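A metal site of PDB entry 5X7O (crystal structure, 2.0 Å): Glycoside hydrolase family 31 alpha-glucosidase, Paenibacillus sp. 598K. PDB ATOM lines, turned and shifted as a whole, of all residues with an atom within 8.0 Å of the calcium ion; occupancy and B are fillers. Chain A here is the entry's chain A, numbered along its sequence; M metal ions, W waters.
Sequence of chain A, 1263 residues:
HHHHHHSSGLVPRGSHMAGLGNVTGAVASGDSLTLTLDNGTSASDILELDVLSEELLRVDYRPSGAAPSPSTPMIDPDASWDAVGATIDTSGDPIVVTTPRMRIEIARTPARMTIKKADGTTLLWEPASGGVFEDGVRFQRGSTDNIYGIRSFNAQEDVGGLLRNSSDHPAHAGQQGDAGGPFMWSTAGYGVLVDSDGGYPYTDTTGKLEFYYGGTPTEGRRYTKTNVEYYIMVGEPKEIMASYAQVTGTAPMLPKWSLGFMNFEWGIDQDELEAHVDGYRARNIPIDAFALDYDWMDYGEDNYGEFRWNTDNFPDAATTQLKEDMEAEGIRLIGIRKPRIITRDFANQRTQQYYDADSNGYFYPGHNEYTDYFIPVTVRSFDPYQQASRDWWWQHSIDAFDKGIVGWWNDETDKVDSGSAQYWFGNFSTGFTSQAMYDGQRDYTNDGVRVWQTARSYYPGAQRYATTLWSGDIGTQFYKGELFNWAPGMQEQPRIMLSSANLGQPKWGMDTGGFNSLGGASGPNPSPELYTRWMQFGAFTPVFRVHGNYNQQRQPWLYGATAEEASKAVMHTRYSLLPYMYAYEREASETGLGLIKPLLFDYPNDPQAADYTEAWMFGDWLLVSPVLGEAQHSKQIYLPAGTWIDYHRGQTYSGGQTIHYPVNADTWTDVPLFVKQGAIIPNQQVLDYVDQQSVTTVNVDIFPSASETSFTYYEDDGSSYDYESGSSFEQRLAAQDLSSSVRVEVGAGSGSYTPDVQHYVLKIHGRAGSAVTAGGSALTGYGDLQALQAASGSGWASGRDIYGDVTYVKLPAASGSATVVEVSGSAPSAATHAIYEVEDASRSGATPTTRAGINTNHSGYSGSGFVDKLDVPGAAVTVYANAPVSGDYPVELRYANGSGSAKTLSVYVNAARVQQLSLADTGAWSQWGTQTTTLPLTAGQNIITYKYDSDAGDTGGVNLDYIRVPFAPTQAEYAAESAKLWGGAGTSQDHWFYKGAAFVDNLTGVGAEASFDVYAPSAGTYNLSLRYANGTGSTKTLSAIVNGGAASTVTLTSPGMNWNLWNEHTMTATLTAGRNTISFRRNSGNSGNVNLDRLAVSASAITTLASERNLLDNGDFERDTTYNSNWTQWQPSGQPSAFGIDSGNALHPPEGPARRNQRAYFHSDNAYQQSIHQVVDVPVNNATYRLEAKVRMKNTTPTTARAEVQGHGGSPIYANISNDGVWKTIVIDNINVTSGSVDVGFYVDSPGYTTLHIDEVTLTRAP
The calcium ion is bound by water W1, OD1 of Asp 1093, O of Ala 998, O of Lys 995, OE1 of Glu 977 and OE2 of Glu 977. The calcium ion has six donor atoms within binding distance. Slightly farther from the calcium ion lies the backbone carbonyl oxygen (O) of Asp 1093 (2.9 Å).
OD2 of Asp 1093 lies within salt-bridge range of NH1 of Arg 1027 (2.7 Å). N of Ala 997 lies close to OE2 of Glu 977. The backbone carbonyl oxygen (O) of Glu 1108 is in hydrogen-bond range of the side-chain amino group (NZ) of Lys 995 (3.3 Å). O of Asp 1093 lies within hydrogen-bond range of N of Ala 976 (3.1 Å).
Within 4 Å of the calcium ion: Glu 977, Lys 995, Ala 998 and Asp 1093. Along chain A the residues within 4 Å of the calcium ion span positions 977 to 1093.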
ATOM      1  N   HIS A 633     -27.984  23.646  16.330  1.00  0.00           N
ATOM      2  CA  HIS A 633     -27.238  22.658  17.160  1.00  0.00           C
ATOM      3  C   HIS A 633     -26.003  22.065  16.489  1.00  0.00           C
ATOM      4  O   HIS A 633     -25.151  21.482  17.166  1.00  0.00           O
ATOM      5  CB  HIS A 633     -28.170  21.527  17.547  1.00  0.00           C
ATOM      6  CG  HIS A 633     -29.396  21.985  18.246  1.00  0.00           C
ATOM      7  ND1 HIS A 633     -29.391  22.428  19.552  1.00  0.00           N
ATOM      8  CD2 HIS A 633     -30.684  22.078  17.829  1.00  0.00           C
ATOM      9  CE1 HIS A 633     -30.613  22.778  19.901  1.00  0.00           C
ATOM     10  NE2 HIS A 633     -31.413  22.575  18.877  1.00  0.00           N
ATOM     11  N   GLU A 973     -18.930  14.837  27.819  1.00  0.00           N
ATOM     12  CA  GLU A 973     -20.324  14.774  27.398  1.00  0.00           C
ATOM     13  C   GLU A 973     -20.486  15.239  25.942  1.00  0.00           C
ATOM     14  O   GLU A 973     -19.758  16.107  25.460  1.00  0.00           O
ATOM     15  CB  GLU A 973     -21.207  15.594  28.335  1.00  0.00           C
ATOM     16  CG  GLU A 973     -20.988  17.085  28.319  1.00  0.00           C
ATOM     17  CD  GLU A 973     -21.916  17.800  29.300  1.00  0.00           C
ATOM     18  OE1 GLU A 973     -23.097  18.052  28.948  1.00  0.00           O
ATOM     19  OE2 GLU A 973     -21.463  18.104  30.424  1.00  0.00           O
ATOM     20  N   TYR A 974     -21.460  14.634  25.281  1.00  0.00           N
ATOM     21  CA  TYR A 974     -21.808  14.933  23.912  1.00  0.00           C
ATOM     22  C   TYR A 974     -23.327  15.056  23.838  1.00  0.00           C
ATOM     23  O   TYR A 974     -24.041  14.126  24.178  1.00  0.00           O
ATOM     24  CB  TYR A 974     -21.284  13.835  22.980  1.00  0.00           C
ATOM     25  CG  TYR A 974     -19.790  13.640  23.065  1.00  0.00           C
ATOM     26  CD1 TYR A 974     -19.219  12.775  24.019  1.00  0.00           C
ATOM     27  CD2 TYR A 974     -18.931  14.317  22.215  1.00  0.00           C
ATOM     28  CE1 TYR A 974     -17.853  12.600  24.116  1.00  0.00           C
ATOM     29  CE2 TYR A 974     -17.555  14.150  22.308  1.00  0.00           C
ATOM     30  CZ  TYR A 974     -17.019  13.291  23.250  1.00  0.00           C
ATOM     31  OH  TYR A 974     -15.661  13.138  23.319  1.00  0.00           O
ATOM     32  N   ALA A 975     -23.814  16.214  23.412  1.00  0.00           N
ATOM     33  CA  ALA A 975     -25.247  16.446  23.262  1.00  0.00           C
ATOM     34  C   ALA A 975     -25.850  15.668  22.071  1.00  0.00           C
ATOM     35  O   ALA A 975     -25.331  15.744  20.961  1.00  0.00           O
ATOM     36  CB  ALA A 975     -25.487  17.944  23.113  1.00  0.00           C
ATOM     37  N   ALA A 976     -26.930  14.934  22.312  1.00  0.00           N
ATOM     38  CA  ALA A 976     -27.646  14.228  21.233  1.00  0.00           C
ATOM     39  C   ALA A 976     -28.126  15.191  20.144  1.00  0.00           C
ATOM     40  O   ALA A 976     -27.935  14.939  18.946  1.00  0.00           O
ATOM     41  CB  ALA A 976     -28.825  13.447  21.803  1.00  0.00           C
ATOM     42  N   GLU A 977     -28.698  16.323  20.559  1.00  0.00           N
ATOM     43  CA  GLU A 977     -29.202  17.326  19.617  1.00  0.00           C
ATOM     44  C   GLU A 977     -28.130  17.916  18.673  1.00  0.00           C
ATOM     45  O   GLU A 977     -28.458  18.384  17.591  1.00  0.00           O
ATOM     46  CB  GLU A 977     -29.956  18.457  20.345  1.00  0.00           C
ATOM     47  CG  GLU A 977     -29.152  19.243  21.370  1.00  0.00           C
ATOM     48  CD  GLU A 977     -29.190  18.647  22.784  1.00  0.00           C
ATOM     49  OE1 GLU A 977     -29.354  17.407  22.936  1.00  0.00           O
ATOM     50  OE2 GLU A 977     -29.028  19.423  23.767  1.00  0.00           O
ATOM     51  N   SER A 978     -26.864  17.892  19.094  1.00  0.00           N
ATOM     52  CA  SER A 978     -25.735  18.310  18.246  1.00  0.00           C
ATOM     53  C   SER A 978     -25.045  17.178  17.462  1.00  0.00           C
ATOM     54  O   SER A 978     -24.084  17.438  16.713  1.00  0.00           O
ATOM     55  CB  SER A 978     -24.685  19.027  19.130  1.00  0.00           C
ATOM     56  OG  SER A 978     -25.214  20.233  19.667  1.00  0.00           O
ATOM     57  N   SER A 988     -36.006  18.308  19.344  1.00  0.00           N
ATOM     58  CA  SER A 988     -37.302  18.656  19.899  1.00  0.00           C
ATOM     59  C   SER A 988     -37.181  19.220  21.320  1.00  0.00           C
ATOM     60  O   SER A 988     -36.230  18.917  22.056  1.00  0.00           O
ATOM     61  CB  SER A 988     -38.183  17.405  19.968  1.00  0.00           C
ATOM     62  OG  SER A 988     -39.458  17.691  20.507  1.00  0.00           O
ATOM     63  N   PHE A 993     -37.634  18.035  31.084  1.00  0.00           N
ATOM     64  CA  PHE A 993     -36.501  17.495  31.825  1.00  0.00           C
ATOM     65  C   PHE A 993     -35.309  17.008  30.990  1.00  0.00           C
ATOM     66  O   PHE A 993     -34.456  16.300  31.508  1.00  0.00           O
ATOM     67  CB  PHE A 993     -36.929  16.442  32.874  1.00  0.00           C
ATOM     68  CG  PHE A 993     -37.773  17.029  33.961  1.00  0.00           C
ATOM     69  CD1 PHE A 993     -37.182  17.780  34.982  1.00  0.00           C
ATOM     70  CD2 PHE A 993     -39.157  16.865  33.963  1.00  0.00           C
ATOM     71  CE1 PHE A 993     -37.961  18.348  35.977  1.00  0.00           C
ATOM     72  CE2 PHE A 993     -39.937  17.432  34.958  1.00  0.00           C
ATOM     73  CZ  PHE A 993     -39.344  18.163  35.966  1.00  0.00           C
ATOM     74  N   TYR A 994     -35.242  17.447  29.726  1.00  0.00           N
ATOM     75  CA  TYR A 994     -34.029  17.272  28.925  1.00  0.00           C
ATOM     76  C   TYR A 994     -32.915  18.208  29.399  1.00  0.00           C
ATOM     77  O   TYR A 994     -33.163  19.274  29.958  1.00  0.00           O
ATOM     78  CB  TYR A 994     -34.311  17.519  27.425  1.00  0.00           C
ATOM     79  CG  TYR A 994     -34.857  18.896  27.077  1.00  0.00           C
ATOM     80  CD1 TYR A 994     -34.008  19.977  26.847  1.00  0.00           C
ATOM     81  CD2 TYR A 994     -36.220  19.103  26.925  1.00  0.00           C
ATOM     82  CE1 TYR A 994     -34.511  21.228  26.516  1.00  0.00           C
ATOM     83  CE2 TYR A 994     -36.740  20.345  26.606  1.00  0.00           C
ATOM     84  CZ  TYR A 994     -35.872  21.412  26.399  1.00  0.00           C
ATOM     85  OH  TYR A 994     -36.381  22.655  26.088  1.00  0.00           O
ATOM     86  N   LYS A 995     -31.676  17.791  29.115  1.00  0.00           N
ATOM     87  CA  LYS A 995     -30.480  18.580  29.388  1.00  0.00           C
ATOM     88  C   LYS A 995     -30.093  19.357  28.160  1.00  0.00           C
ATOM     89  O   LYS A 995     -30.444  18.989  27.039  1.00  0.00           O
ATOM     90  CB  LYS A 995     -29.336  17.642  29.791  1.00  0.00           C
ATOM     91  CG  LYS A 995     -29.646  16.752  30.974  1.00  0.00           C
ATOM     92  CD  LYS A 995     -30.022  17.551  32.210  1.00  0.00           C
ATOM     93  CE  LYS A 995     -30.250  16.631  33.387  1.00  0.00           C
ATOM     94  NZ  LYS A 995     -30.340  17.403  34.659  1.00  0.00           N
ATOM     95  N   GLY A 996     -29.405  20.481  28.372  1.00  0.00           N
ATOM     96  CA  GLY A 996     -29.024  21.363  27.273  1.00  0.00           C
ATOM     97  C   GLY A 996     -30.213  21.969  26.561  1.00  0.00           C
ATOM     98  O   GLY A 996     -31.311  22.109  27.122  1.00  0.00           O
ATOM     99  N   ALA A 997     -30.019  22.303  25.290  1.00  0.00           N
ATOM    100  CA  ALA A 997     -30.983  23.089  24.532  1.00  0.00           C
ATOM    101  C   ALA A 997     -32.169  22.296  23.961  1.00  0.00           C
ATOM    102  O   ALA A 997     -33.181  22.885  23.602  1.00  0.00           O
ATOM    103  CB  ALA A 997     -30.270  23.844  23.418  1.00  0.00           C
ATOM    104  N   ALA A 998     -32.029  20.969  23.863  1.00  0.00           N
ATOM    105  CA  ALA A 998     -33.063  20.124  23.258  1.00  0.00           C
ATOM    106  C   ALA A 998     -32.758  18.623  23.512  1.00  0.00           C
ATOM    107  O   ALA A 998     -31.851  18.287  24.287  1.00  0.00           O
ATOM    108  CB  ALA A 998     -33.156  20.404  21.746  1.00  0.00           C
ATOM    109  N   PHE A 999     -33.501  17.750  22.849  1.00  0.00           N
ATOM    110  CA  PHE A 999     -33.197  16.324  22.804  1.00  0.00           C
ATOM    111  C   PHE A 999     -33.518  15.803  21.396  1.00  0.00           C
ATOM    112  O   PHE A 999     -34.040  16.557  20.562  1.00  0.00           O
ATOM    113  CB  PHE A 999     -33.991  15.559  23.874  1.00  0.00           C
ATOM    114  CG  PHE A 999     -35.476  15.694  23.740  1.00  0.00           C
ATOM    115  CD1 PHE A 999     -36.138  16.736  24.388  1.00  0.00           C
ATOM    116  CD2 PHE A 999     -36.222  14.775  22.996  1.00  0.00           C
ATOM    117  CE1 PHE A 999     -37.513  16.877  24.269  1.00  0.00           C
ATOM    118  CE2 PHE A 999     -37.603  14.909  22.873  1.00  0.00           C
ATOM    119  CZ  PHE A 999     -38.249  15.974  23.510  1.00  0.00           C
ATOM    120  N   VAL A1000     -33.225  14.531  21.140  1.00  0.00           N
ATOM    121  CA  VAL A1000     -33.435  13.913  19.823  1.00  0.00           C
ATOM    122  C   VAL A1000     -34.631  12.983  19.890  1.00  0.00           C
ATOM    123  O   VAL A1000     -34.741  12.178  20.806  1.00  0.00           O
ATOM    124  CB  VAL A1000     -32.188  13.167  19.340  1.00  0.00           C
ATOM    125  CG1 VAL A1000     -32.505  12.258  18.150  1.00  0.00           C
ATOM    126  CG2 VAL A1000     -31.085  14.159  18.971  1.00  0.00           C
ATOM    127  N   ARG A1027     -28.249   8.980  28.103  1.00  0.00           N
ATOM    128  CA  ARG A1027     -29.495   9.462  28.718  1.00  0.00           C
ATOM    129  C   ARG A1027     -30.634   9.401  27.693  1.00  0.00           C
ATOM    130  O   ARG A1027     -30.515   9.954  26.611  1.00  0.00           O
ATOM    131  CB  ARG A1027     -29.302  10.878  29.239  1.00  0.00           C
ATOM    132  CG  ARG A1027     -30.440  11.410  30.092  1.00  0.00           C
ATOM    133  CD  ARG A1027     -30.055  12.737  30.749  1.00  0.00           C
ATOM    134  NE  ARG A1027     -30.916  13.043  31.881  1.00  0.00           N
ATOM    135  CZ  ARG A1027     -32.005  13.814  31.864  1.00  0.00           C
ATOM    136  NH1 ARG A1027     -32.439  14.404  30.758  1.00  0.00           N
ATOM    137  NH2 ARG A1027     -32.679  14.003  33.003  1.00  0.00           N
ATOM    138  N   TRP A1062     -36.360  10.459  32.394  1.00  0.00           N
ATOM    139  CA  TRP A1062     -35.141  10.108  31.688  1.00  0.00           C
ATOM    140  C   TRP A1062     -34.360   9.114  32.530  1.00  0.00           C
ATOM    141  O   TRP A1062     -34.444   9.144  33.756  1.00  0.00           O
ATOM    142  CB  TRP A1062     -34.332  11.374  31.412  1.00  0.00           C
ATOM    143  CG  TRP A1062     -35.094  12.355  30.569  1.00  0.00           C
ATOM    144  CD1 TRP A1062     -35.972  13.296  31.010  1.00  0.00           C
ATOM    145  CD2 TRP A1062     -35.045  12.490  29.141  1.00  0.00           C
ATOM    146  NE1 TRP A1062     -36.476  14.008  29.952  1.00  0.00           N
ATOM    147  CE2 TRP A1062     -35.924  13.541  28.799  1.00  0.00           C
ATOM    148  CE3 TRP A1062     -34.341  11.827  28.122  1.00  0.00           C
ATOM    149  CZ2 TRP A1062     -36.116  13.947  27.475  1.00  0.00           C
ATOM    150  CZ3 TRP A1062     -34.533  12.225  26.809  1.00  0.00           C
ATOM    151  CH2 TRP A1062     -35.412  13.289  26.492  1.00  0.00           C
ATOM    152  N   LEU A1092     -33.348  10.433  22.775  1.00  0.00           N
ATOM    153  CA  LEU A1092     -31.976  10.484  23.240  1.00  0.00           C
ATOM    154  C   LEU A1092     -31.583  11.914  23.608  1.00  0.00           C
ATOM    155  O   LEU A1092     -31.949  12.867  22.939  1.00  0.00           O
ATOM    156  CB  LEU A1092     -31.020   9.946  22.164  1.00  0.00           C
ATOM    157  CG  LEU A1092     -31.346   8.539  21.612  1.00  0.00           C
ATOM    158  CD1 LEU A1092     -30.304   8.117  20.582  1.00  0.00           C
ATOM    159  CD2 LEU A1092     -31.417   7.505  22.715  1.00  0.00           C
ATOM    160  N   ASP A1093     -30.796  12.057  24.678  1.00  0.00           N
ATOM    161  CA  ASP A1093     -30.494  13.386  25.205  1.00  0.00           C
ATOM    162  C   ASP A1093     -29.004  13.711  25.243  1.00  0.00           C
ATOM    163  O   ASP A1093     -28.615  14.828  24.881  1.00  0.00           O
ATOM    164  CB  ASP A1093     -31.085  13.496  26.600  1.00  0.00           C
ATOM    165  CG  ASP A1093     -31.153  14.909  27.124  1.00  0.00           C
ATOM    166  OD1 ASP A1093     -31.097  15.853  26.319  1.00  0.00           O
ATOM    167  OD2 ASP A1093     -31.299  15.090  28.359  1.00  0.00           O
ATOM    168  N   ARG A1094     -28.189  12.765  25.674  1.00  0.00           N
ATOM    169  CA  ARG A1094     -26.768  13.016  25.937  1.00  0.00           C
ATOM    170  C   ARG A1094     -26.001  11.700  26.078  1.00  0.00           C
ATOM    171  O   ARG A1094     -26.504  10.761  26.672  1.00  0.00           O
ATOM    172  CB  ARG A1094     -26.623  13.829  27.242  1.00  0.00           C
ATOM    173  CG  ARG A1094     -25.196  14.178  27.654  1.00  0.00           C
ATOM    174  CD  ARG A1094     -24.587  13.187  28.633  1.00  0.00           C
ATOM    175  NE  ARG A1094     -25.344  13.145  29.887  1.00  0.00           N
ATOM    176  CZ  ARG A1094     -25.849  12.057  30.476  1.00  0.00           C
ATOM    177  NH1 ARG A1094     -25.701  10.832  29.979  1.00  0.00           N
ATOM    178  NH2 ARG A1094     -26.526  12.204  31.621  1.00  0.00           N
ATOM    179  N   LEU A1095     -24.784  11.680  25.539  1.00  0.00           N
ATOM    180  CA  LEU A1095     -23.834  10.579  25.718  1.00  0.00           C
ATOM    181  C   LEU A1095     -22.687  11.039  26.606  1.00  0.00           C
ATOM    182  O   LEU A1095     -21.980  11.990  26.264  1.00  0.00           O
ATOM    183  CB  LEU A1095     -23.256  10.139  24.378  1.00  0.00           C
ATOM    184  CG  LEU A1095     -22.317   8.925  24.415  1.00  0.00           C
ATOM    185  CD1 LEU A1095     -23.069   7.688  24.869  1.00  0.00           C
ATOM    186  CD2 LEU A1095     -21.676   8.668  23.064  1.00  0.00           C
ATOM    187  N   GLU A1108     -25.259  19.134  34.748  1.00  0.00           N
ATOM    188  CA  GLU A1108     -26.559  18.497  34.919  1.00  0.00           C
ATOM    189  C   GLU A1108     -27.010  18.491  36.376  1.00  0.00           C
ATOM    190  O   GLU A1108     -27.786  17.632  36.765  1.00  0.00           O
ATOM    191  CB  GLU A1108     -26.491  17.065  34.358  1.00  0.00           C
ATOM    192  CG  GLU A1108     -26.165  17.015  32.871  1.00  0.00           C
ATOM    193  CD  GLU A1108     -26.315  15.645  32.225  1.00  0.00           C
ATOM    194  OE1 GLU A1108     -26.635  14.649  32.916  1.00  0.00           O
ATOM    195  OE2 GLU A1108     -26.105  15.546  30.982  1.00  0.00           O
HETATM  196 CA    CA M   1     -29.959  17.403  25.298  1.00  0.00          CA
HETATM  197  O   HOH W   1     -28.041  17.259  26.048  1.00  0.00           O
